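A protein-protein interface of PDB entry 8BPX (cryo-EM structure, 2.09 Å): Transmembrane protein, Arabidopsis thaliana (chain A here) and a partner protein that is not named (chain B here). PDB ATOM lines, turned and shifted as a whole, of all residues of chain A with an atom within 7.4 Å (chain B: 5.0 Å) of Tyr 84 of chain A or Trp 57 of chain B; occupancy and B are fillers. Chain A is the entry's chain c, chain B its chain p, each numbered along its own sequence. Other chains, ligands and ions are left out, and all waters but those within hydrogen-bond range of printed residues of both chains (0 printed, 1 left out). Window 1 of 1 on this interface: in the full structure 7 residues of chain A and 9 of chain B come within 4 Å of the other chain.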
ATOM      1  N   GLN A  60      14.607 -19.935 -12.878  1.00  0.00           N
ATOM      2  CA  GLN A  60      15.445 -19.123 -12.002  1.00  0.00           C
ATOM      3  C   GLN A  60      14.558 -18.490 -10.940  1.00  0.00           C
ATOM      4  O   GLN A  60      13.648 -17.721 -11.266  1.00  0.00           O
ATOM      5  CB  GLN A  60      16.196 -18.042 -12.787  1.00  0.00           C
ATOM      6  CG  GLN A  60      17.121 -18.573 -13.873  1.00  0.00           C
ATOM      7  CD  GLN A  60      18.351 -19.270 -13.329  1.00  0.00           C
ATOM      8  OE1 GLN A  60      18.944 -18.834 -12.350  1.00  0.00           O
ATOM      9  NE2 GLN A  60      18.731 -20.369 -13.963  1.00  0.00           N
ATOM     10  N   ARG A  61      14.828 -18.807  -9.674  1.00  0.00           N
ATOM     11  CA  ARG A  61      14.046 -18.308  -8.542  1.00  0.00           C
ATOM     12  C   ARG A  61      14.965 -17.505  -7.631  1.00  0.00           C
ATOM     13  O   ARG A  61      15.609 -18.065  -6.732  1.00  0.00           O
ATOM     14  CB  ARG A  61      13.380 -19.454  -7.785  1.00  0.00           C
ATOM     15  CG  ARG A  61      12.833 -20.569  -8.665  1.00  0.00           C
ATOM     16  CD  ARG A  61      11.721 -20.073  -9.579  1.00  0.00           C
ATOM     17  NE  ARG A  61      10.507 -19.739  -8.844  1.00  0.00           N
ATOM     18  CZ  ARG A  61       9.615 -20.622  -8.419  1.00  0.00           C
ATOM     19  NH1 ARG A  61       9.759 -21.914  -8.644  1.00  0.00           N
ATOM     20  NH2 ARG A  61       8.552 -20.194  -7.746  1.00  0.00           N
ATOM     21  N   PRO A  62      15.065 -16.191  -7.835  1.00  0.00           N
ATOM     22  CA  PRO A  62      15.984 -15.390  -7.011  1.00  0.00           C
ATOM     23  C   PRO A  62      15.611 -15.343  -5.538  1.00  0.00           C
ATOM     24  O   PRO A  62      16.476 -15.058  -4.703  1.00  0.00           O
ATOM     25  CB  PRO A  62      15.901 -13.997  -7.647  1.00  0.00           C
ATOM     26  CG  PRO A  62      15.297 -14.211  -8.993  1.00  0.00           C
ATOM     27  CD  PRO A  62      14.388 -15.373  -8.855  1.00  0.00           C
ATOM     28  N   THR A  80      20.251 -17.757  -6.311  1.00  0.00           N
ATOM     29  CA  THR A  80      21.510 -17.804  -7.040  1.00  0.00           C
ATOM     30  C   THR A  80      21.880 -16.472  -7.683  1.00  0.00           C
ATOM     31  O   THR A  80      23.049 -16.270  -8.027  1.00  0.00           O
ATOM     32  CB  THR A  80      21.447 -18.909  -8.111  1.00  0.00           C
ATOM     33  OG1 THR A  80      21.142 -20.155  -7.482  1.00  0.00           O
ATOM     34  CG2 THR A  80      22.779 -19.068  -8.845  1.00  0.00           C
ATOM     35  N   LYS A  81      20.935 -15.546  -7.810  1.00  0.00           N
ATOM     36  CA  LYS A  81      21.170 -14.278  -8.483  1.00  0.00           C
ATOM     37  C   LYS A  81      21.507 -13.144  -7.524  1.00  0.00           C
ATOM     38  O   LYS A  81      21.385 -11.974  -7.902  1.00  0.00           O
ATOM     39  CB  LYS A  81      19.952 -13.903  -9.327  1.00  0.00           C
ATOM     40  CG  LYS A  81      19.635 -14.899 -10.423  1.00  0.00           C
ATOM     41  CD  LYS A  81      20.826 -15.121 -11.322  1.00  0.00           C
ATOM     42  CE  LYS A  81      20.447 -15.949 -12.535  1.00  0.00           C
ATOM     43  NZ  LYS A  81      21.425 -15.809 -13.635  1.00  0.00           N
ATOM     44  N   ASP A  82      21.946 -13.455  -6.303  1.00  0.00           N
ATOM     45  CA  ASP A  82      22.163 -12.409  -5.309  1.00  0.00           C
ATOM     46  C   ASP A  82      23.274 -11.457  -5.725  1.00  0.00           C
ATOM     47  O   ASP A  82      23.195 -10.251  -5.468  1.00  0.00           O
ATOM     48  CB  ASP A  82      22.476 -13.030  -3.953  1.00  0.00           C
ATOM     49  CG  ASP A  82      21.231 -13.426  -3.209  1.00  0.00           C
ATOM     50  OD1 ASP A  82      20.206 -12.744  -3.389  1.00  0.00           O
ATOM     51  OD2 ASP A  82      21.271 -14.416  -2.454  1.00  0.00           O
ATOM     52  N   ASP A  83      24.320 -11.980  -6.355  1.00  0.00           N
ATOM     53  CA  ASP A  83      25.438 -11.156  -6.799  1.00  0.00           C
ATOM     54  C   ASP A  83      25.219 -10.747  -8.255  1.00  0.00           C
ATOM     55  O   ASP A  83      25.899 -11.191  -9.182  1.00  0.00           O
ATOM     56  CB  ASP A  83      26.750 -11.904  -6.600  1.00  0.00           C
ATOM     57  CG  ASP A  83      27.947 -11.000  -6.685  1.00  0.00           C
ATOM     58  OD1 ASP A  83      27.761  -9.777  -6.858  1.00  0.00           O
ATOM     59  OD2 ASP A  83      29.081 -11.504  -6.555  1.00  0.00           O
ATOM     60  N   TYR A  84      24.233  -9.869  -8.442  1.00  0.00           N
ATOM     61  CA  TYR A  84      23.886  -9.411  -9.781  1.00  0.00           C
ATOM     62  C   TYR A  84      24.951  -8.508 -10.383  1.00  0.00           C
ATOM     63  O   TYR A  84      24.900  -8.236 -11.587  1.00  0.00           O
ATOM     64  CB  TYR A  84      22.528  -8.702  -9.759  1.00  0.00           C
ATOM     65  CG  TYR A  84      22.349  -7.682  -8.659  1.00  0.00           C
ATOM     66  CD1 TYR A  84      23.051  -6.485  -8.673  1.00  0.00           C
ATOM     67  CD2 TYR A  84      21.494  -7.928  -7.591  1.00  0.00           C
ATOM     68  CE1 TYR A  84      22.893  -5.559  -7.675  1.00  0.00           C
ATOM     69  CE2 TYR A  84      21.331  -7.004  -6.584  1.00  0.00           C
ATOM     70  CZ  TYR A  84      22.031  -5.822  -6.629  1.00  0.00           C
ATOM     71  OH  TYR A  84      21.872  -4.896  -5.631  1.00  0.00           O
ATOM     72  N   GLU A  85      25.911  -8.047  -9.581  1.00  0.00           N
ATOM     73  CA  GLU A  85      27.008  -7.248 -10.105  1.00  0.00           C
ATOM     74  C   GLU A  85      27.900  -8.049 -11.045  1.00  0.00           C
ATOM     75  O   GLU A  85      28.544  -7.472 -11.924  1.00  0.00           O
ATOM     76  CB  GLU A  85      27.836  -6.688  -8.952  1.00  0.00           C
ATOM     77  CG  GLU A  85      28.121  -5.206  -9.028  1.00  0.00           C
ATOM     78  CD  GLU A  85      26.876  -4.361  -8.923  1.00  0.00           C
ATOM     79  OE1 GLU A  85      25.886  -4.829  -8.330  1.00  0.00           O
ATOM     80  OE2 GLU A  85      26.895  -3.214  -9.409  1.00  0.00           O
ATOM     81  N   LYS A  86      27.992  -9.335 -10.820  1.00  0.00           N
ATOM     82  CA  LYS A  86      28.796 -10.240 -11.658  1.00  0.00           C
ATOM     83  C   LYS A  86      27.992 -10.823 -12.842  1.00  0.00           C
ATOM     84  O   LYS A  86      28.525 -11.608 -13.564  1.00  0.00           O
ATOM     85  CB  LYS A  86      29.330 -11.244 -10.632  1.00  0.00           C
ATOM     86  CG  LYS A  86      30.008 -10.662  -9.408  1.00  0.00           C
ATOM     87  CD  LYS A  86      31.366 -10.074  -9.645  1.00  0.00           C
ATOM     88  CE  LYS A  86      32.239 -10.162  -8.412  1.00  0.00           C
ATOM     89  NZ  LYS A  86      32.262 -11.542  -7.874  1.00  0.00           N
ATOM     90  N   GLU A  87      26.727 -10.489 -12.988  1.00  0.00           N
ATOM     91  CA  GLU A  87      25.946 -10.943 -14.171  1.00  0.00           C
ATOM     92  C   GLU A  87      26.613 -10.544 -15.501  1.00  0.00           C
ATOM     93  O   GLU A  87      27.193  -9.462 -15.567  1.00  0.00           O
ATOM     94  CB  GLU A  87      24.518 -10.433 -14.107  1.00  0.00           C
ATOM     95  CG  GLU A  87      23.673 -11.173 -13.106  1.00  0.00           C
ATOM     96  CD  GLU A  87      23.699 -12.663 -13.329  1.00  0.00           C
ATOM     97  OE1 GLU A  87      24.314 -13.354 -12.518  1.00  0.00           O
ATOM     98  OE2 GLU A  87      23.136 -13.119 -14.334  1.00  0.00           O
ATOM     99  N   HIS A  88      26.565 -11.418 -16.489  1.00  0.00           N
ATOM    100  CA  HIS A  88      27.106 -11.104 -17.852  1.00  0.00           C
ATOM    101  C   HIS A  88      26.243 -11.733 -18.953  1.00  0.00           C
ATOM    102  O   HIS A  88      25.188 -12.212 -18.615  1.00  0.00           O
ATOM    103  CB  HIS A  88      28.581 -11.420 -17.941  1.00  0.00           C
ATOM    104  CG  HIS A  88      28.963 -12.849 -17.883  1.00  0.00           C
ATOM    105  ND1 HIS A  88      28.985 -13.643 -19.002  1.00  0.00           N
ATOM    106  CD2 HIS A  88      29.431 -13.594 -16.870  1.00  0.00           C
ATOM    107  CE1 HIS A  88      29.395 -14.839 -18.664  1.00  0.00           C
ATOM    108  NE2 HIS A  88      29.681 -14.827 -17.372  1.00  0.00           N
ATOM    109  N   GLU B  53      22.341  -6.847 -18.351  1.00  0.00           N
ATOM    110  CA  GLU B  53      22.179  -8.073 -17.511  1.00  0.00           C
ATOM    111  C   GLU B  53      22.221  -7.705 -15.985  1.00  0.00           C
ATOM    112  O   GLU B  53      21.322  -8.134 -15.323  1.00  0.00           O
ATOM    113  CB  GLU B  53      23.160  -9.158 -17.981  1.00  0.00           C
ATOM    114  CG  GLU B  53      22.515 -10.500 -18.123  1.00  0.00           C
ATOM    115  CD  GLU B  53      21.318 -10.497 -19.052  1.00  0.00           C
ATOM    116  OE1 GLU B  53      21.386  -9.838 -20.096  1.00  0.00           O
ATOM    117  OE2 GLU B  53      20.319 -11.133 -18.709  1.00  0.00           O
ATOM    118  N   LYS B  54      23.117  -6.802 -15.566  1.00  0.00           N
ATOM    119  CA  LYS B  54      23.183  -6.276 -14.142  1.00  0.00           C
ATOM    120  C   LYS B  54      21.875  -5.612 -13.705  1.00  0.00           C
ATOM    121  O   LYS B  54      21.331  -6.080 -12.769  1.00  0.00           O
ATOM    122  CB  LYS B  54      24.437  -5.411 -13.971  1.00  0.00           C
ATOM    123  CG  LYS B  54      25.751  -6.143 -14.221  1.00  0.00           C
ATOM    124  CD  LYS B  54      26.974  -5.306 -13.927  1.00  0.00           C
ATOM    125  CE  LYS B  54      28.225  -5.715 -14.671  1.00  0.00           C
ATOM    126  NZ  LYS B  54      28.556  -7.150 -14.531  1.00  0.00           N
ATOM    127  N   VAL B  55      21.342  -4.703 -14.526  1.00  0.00           N
ATOM    128  CA  VAL B  55      20.067  -4.008 -14.270  1.00  0.00           C
ATOM    129  C   VAL B  55      18.961  -5.029 -14.209  1.00  0.00           C
ATOM    130  O   VAL B  55      18.260  -4.965 -13.224  1.00  0.00           O
ATOM    131  CB  VAL B  55      19.813  -2.851 -15.268  1.00  0.00           C
ATOM    132  CG1 VAL B  55      18.445  -2.232 -15.142  1.00  0.00           C
ATOM    133  CG2 VAL B  55      20.908  -1.802 -15.202  1.00  0.00           C
ATOM    134  N   LYS B  56      18.875  -5.918 -15.210  1.00  0.00           N
ATOM    135  CA  LYS B  56      17.829  -6.925 -15.292  1.00  0.00           C
ATOM    136  C   LYS B  56      17.752  -7.628 -13.914  1.00  0.00           C
ATOM    137  O   LYS B  56      16.706  -7.570 -13.308  1.00  0.00           O
ATOM    138  CB  LYS B  56      18.078  -7.909 -16.454  1.00  0.00           C
ATOM    139  CG  LYS B  56      17.022  -8.958 -16.733  1.00  0.00           C
ATOM    140  CD  LYS B  56      17.391  -9.917 -17.849  1.00  0.00           C
ATOM    141  CE  LYS B  56      17.380  -9.313 -19.238  1.00  0.00           C
ATOM    142  NZ  LYS B  56      18.700  -8.811 -19.689  1.00  0.00           N
ATOM    143  N   TRP B  57      18.867  -8.157 -13.476  1.00  0.00           N
ATOM    144  CA  TRP B  57      18.946  -8.949 -12.225  1.00  0.00           C
ATOM    145  C   TRP B  57      18.753  -8.124 -10.956  1.00  0.00           C
ATOM    146  O   TRP B  57      18.082  -8.639 -10.133  1.00  0.00           O
ATOM    147  CB  TRP B  57      20.188  -9.826 -12.244  1.00  0.00           C
ATOM    148  CG  TRP B  57      19.928 -10.949 -13.198  1.00  0.00           C
ATOM    149  CD1 TRP B  57      20.509 -11.148 -14.416  1.00  0.00           C
ATOM    150  CD2 TRP B  57      18.916 -11.964 -13.070  1.00  0.00           C
ATOM    151  NE1 TRP B  57      19.964 -12.240 -15.024  1.00  0.00           N
ATOM    152  CE2 TRP B  57      18.992 -12.770 -14.225  1.00  0.00           C
ATOM    153  CE3 TRP B  57      17.977 -12.289 -12.085  1.00  0.00           C
ATOM    154  CZ2 TRP B  57      18.161 -13.869 -14.428  1.00  0.00           C
ATOM    155  CZ3 TRP B  57      17.158 -13.375 -12.285  1.00  0.00           C
ATOM    156  CH2 TRP B  57      17.257 -14.163 -13.435  1.00  0.00           C
ATOM    157  N   CYS B  58      19.236  -6.885 -10.900  1.00  0.00           N
ATOM    158  CA  CYS B  58      19.020  -6.005  -9.721  1.00  0.00           C
ATOM    159  C   CYS B  58      17.516  -5.713  -9.589  1.00  0.00           C
ATOM    160  O   CYS B  58      17.017  -6.016  -8.539  1.00  0.00           O
ATOM    161  CB  CYS B  58      19.971  -4.815  -9.761  1.00  0.00           C
ATOM    162  SG  CYS B  58      19.855  -3.658  -8.379  1.00  0.00           S
ATOM    163  N   TYR B  59      16.825  -5.287 -10.652  1.00  0.00           N
ATOM    164  CA  TYR B  59      15.362  -5.142 -10.676  1.00  0.00           C
ATOM    165  C   TYR B  59      14.730  -6.397 -10.091  1.00  0.00           C
ATOM    166  O   TYR B  59      13.956  -6.211  -9.190  1.00  0.00           O
ATOM    167  CB  TYR B  59      14.788  -4.768 -12.058  1.00  0.00           C
ATOM    168  CG  TYR B  59      13.340  -4.407 -12.118  1.00  0.00           C
ATOM    169  CD1 TYR B  59      12.943  -3.099 -11.912  1.00  0.00           C
ATOM    170  CD2 TYR B  59      12.384  -5.363 -12.406  1.00  0.00           C
ATOM    171  CE1 TYR B  59      11.618  -2.746 -11.985  1.00  0.00           C
ATOM    172  CE2 TYR B  59      11.049  -5.023 -12.486  1.00  0.00           C
ATOM    173  CZ  TYR B  59      10.673  -3.711 -12.270  1.00  0.00           C
ATOM    174  OH  TYR B  59       9.378  -3.329 -12.332  1.00  0.00           O
ATOM    175  N   ARG B  60      15.052  -7.562 -10.627  1.00  0.00           N
ATOM    176  CA  ARG B  60      14.488  -8.851 -10.231  1.00  0.00           C
ATOM    177  C   ARG B  60      14.845  -9.201  -8.783  1.00  0.00           C
ATOM    178  O   ARG B  60      14.054  -9.788  -8.133  1.00  0.00           O
ATOM    179  CB  ARG B  60      14.978  -9.944 -11.189  1.00  0.00           C
ATOM    180  CG  ARG B  60      14.348  -9.876 -12.573  1.00  0.00           C
ATOM    181  CD  ARG B  60      14.998 -10.726 -13.635  1.00  0.00           C
ATOM    182  NE  ARG B  60      14.310 -10.546 -14.902  1.00  0.00           N
ATOM    183  CZ  ARG B  60      14.454 -11.326 -15.964  1.00  0.00           C
ATOM    184  NH1 ARG B  60      15.279 -12.352 -15.942  1.00  0.00           N
ATOM    185  NH2 ARG B  60      13.765 -11.064 -17.051  1.00  0.00           N
ATOM    186  N   VAL B  61      16.077  -8.927  -8.404  1.00  0.00           N
ATOM    187  CA  VAL B  61      16.421  -9.361  -7.056  1.00  0.00           C
ATOM    188  C   VAL B  61      15.901  -8.378  -6.012  1.00  0.00           C
ATOM    189  O   VAL B  61      15.402  -8.783  -4.961  1.00  0.00           O
ATOM    190  CB  VAL B  61      17.944  -9.577  -6.944  1.00  0.00           C
ATOM    191  CG1 VAL B  61      18.401  -9.538  -5.493  1.00  0.00           C
ATOM    192  CG2 VAL B  61      18.340 -10.897  -7.589  1.00  0.00           C
ATOM    193  N   GLU B  62      15.981  -7.078  -6.283  1.00  0.00           N
ATOM    194  CA  GLU B  62      15.679  -6.079  -5.268  1.00  0.00           C
ATOM    195  C   GLU B  62      14.210  -5.679  -5.196  1.00  0.00           C
ATOM    196  O   GLU B  62      13.818  -5.031  -4.221  1.00  0.00           O
ATOM    197  CB  GLU B  62      16.536  -4.832  -5.491  1.00  0.00           C
ATOM    198  CG  GLU B  62      18.019  -5.125  -5.555  1.00  0.00           C
ATOM    199  CD  GLU B  62      18.630  -5.440  -4.199  1.00  0.00           C
ATOM    200  OE1 GLU B  62      17.886  -5.640  -3.223  1.00  0.00           O
ATOM    201  OE2 GLU B  62      19.871  -5.491  -4.112  1.00  0.00           O
ATOM    202  N   LYS B  69      18.495   0.634  -5.097  1.00  0.00           N
ATOM    203  CA  LYS B  69      19.581  -0.326  -5.260  1.00  0.00           C
ATOM    204  C   LYS B  69      20.172  -0.354  -6.669  1.00  0.00           C
ATOM    205  O   LYS B  69      21.378  -0.575  -6.808  1.00  0.00           O
ATOM    206  CB  LYS B  69      19.109  -1.731  -4.878  1.00  0.00           C
ATOM    207  CG  LYS B  69      18.655  -1.856  -3.430  1.00  0.00           C
ATOM    208  CD  LYS B  69      19.802  -1.605  -2.469  1.00  0.00           C
ATOM    209  CE  LYS B  69      19.391  -1.795  -1.018  1.00  0.00           C
ATOM    210  NZ  LYS B  69      20.506  -1.526  -0.067  1.00  0.00           N
ATOM    211  N   LEU B  73      23.824   1.158 -11.258  1.00  0.00           N
ATOM    212  CA  LEU B  73      23.810   0.294 -12.435  1.00  0.00           C
ATOM    213  C   LEU B  73      22.988   0.910 -13.557  1.00  0.00           C
ATOM    214  O   LEU B  73      23.376   0.840 -14.728  1.00  0.00           O
ATOM    215  CB  LEU B  73      23.273  -1.087 -12.071  1.00  0.00           C
ATOM    216  CG  LEU B  73      24.216  -1.994 -11.281  1.00  0.00           C
ATOM    217  CD1 LEU B  73      23.583  -3.352 -11.042  1.00  0.00           C
ATOM    218  CD2 LEU B  73      25.557  -2.132 -11.988  1.00  0.00           C
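Trp 57 of chain B touches four residues of chain A.
Of the printed residues of chain B, Pro 62 of chain A touches Trp 57 and Val 61.
Printed residues of chain A within 4 Å of Lys 54 of chain B: Tyr 84, Glu 85 and Glu 87.
Of the printed residues of chain A, Cys 58 of chain B touches Tyr 84 (3.5 Å).
Printed residues of chain A within 4 Å of Glu 62 of chain B: Tyr 84.
Asp 82 of chain A touches none of the printed residues of chain B.
The nearest printed residue of chain A that does not touch Glu 62 of chain B is Asp 82 of chain A (6.0 Å).
The side-chain hydroxyl of Tyr 84 of chain A sits close to the side-chain sulfur of Cys 58 of chain B, at 3.6 Å.
OH of Tyr 84 of chain A lies within hydrogen-bond range of OE2 of Glu 62 of chain B (2.6 Å).
O of Glu 85 of chain A lies within hydrogen-bond range of NZ of Lys 54 of chain B.
NZ of Lys 54 of chain B is in hydrogen-bond range of O of Glu 87 of chain A, 2.9 Å away.
NE1 of Trp 57 of chain B lies close to OE2 of Glu 87 of chain A (3.4 Å).
Hydrophobic or aromatic side chains of chain B within 4 Å of the printed part of chain A: Trp 57, Val 61 and Leu 73.
Along chain B the printed residues that touch a printed residue of chain A span positions 53 to 73.
Hydrophobic or aromatic side chains of chain A within 4 Å of the printed part of chain B: Pro 62 and Tyr 84.
Among the printed residues, no Asp or Glu carboxylate lies within 4 Å of a Lys or Arg side-chain nitrogen of the other chain.
The side-chain amino group (NZ) of Lys 81 of chain A is in salt-bridge range of the side-chain carboxylate (OE2) of Glu 87 of chain A, at 3.3 Å.
The side-chain carboxylate of Glu 53 of chain B is in salt-bridge range of the side-chain amino group of Lys 56 of chain B, 2.9 Å away.
SG of Cys 58 of chain B sits close to O of Lys 69 of chain B (3.8 Å).
Among the printed residues, merely in contact across the chains: Glu 85 of chain A with Leu 73 of chain B (3.1 Å), His 88 of chain A with Glu 53 of chain B (3.2 Å), Lys 81 of chain A with Val 61 of chain B (3.2 Å), Lys 81 of chain A with Trp 57 of chain B (3.5 Å), Tyr 84 of chain A with Lys 54 of chain B (3.5 Å), Tyr 84 of chain A with Trp 57 of chain B (3.6 Å), Pro 62 of chain A with Trp 57 of chain B (3.9 Å), Pro 62 of chain A with Val 61 of chain B (3.9 Å), Tyr 84 of chain A with Leu 73 of chain B (3.96 Å) and Tyr 84 of chain A with Val 61 of chain B (3.97 Å).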
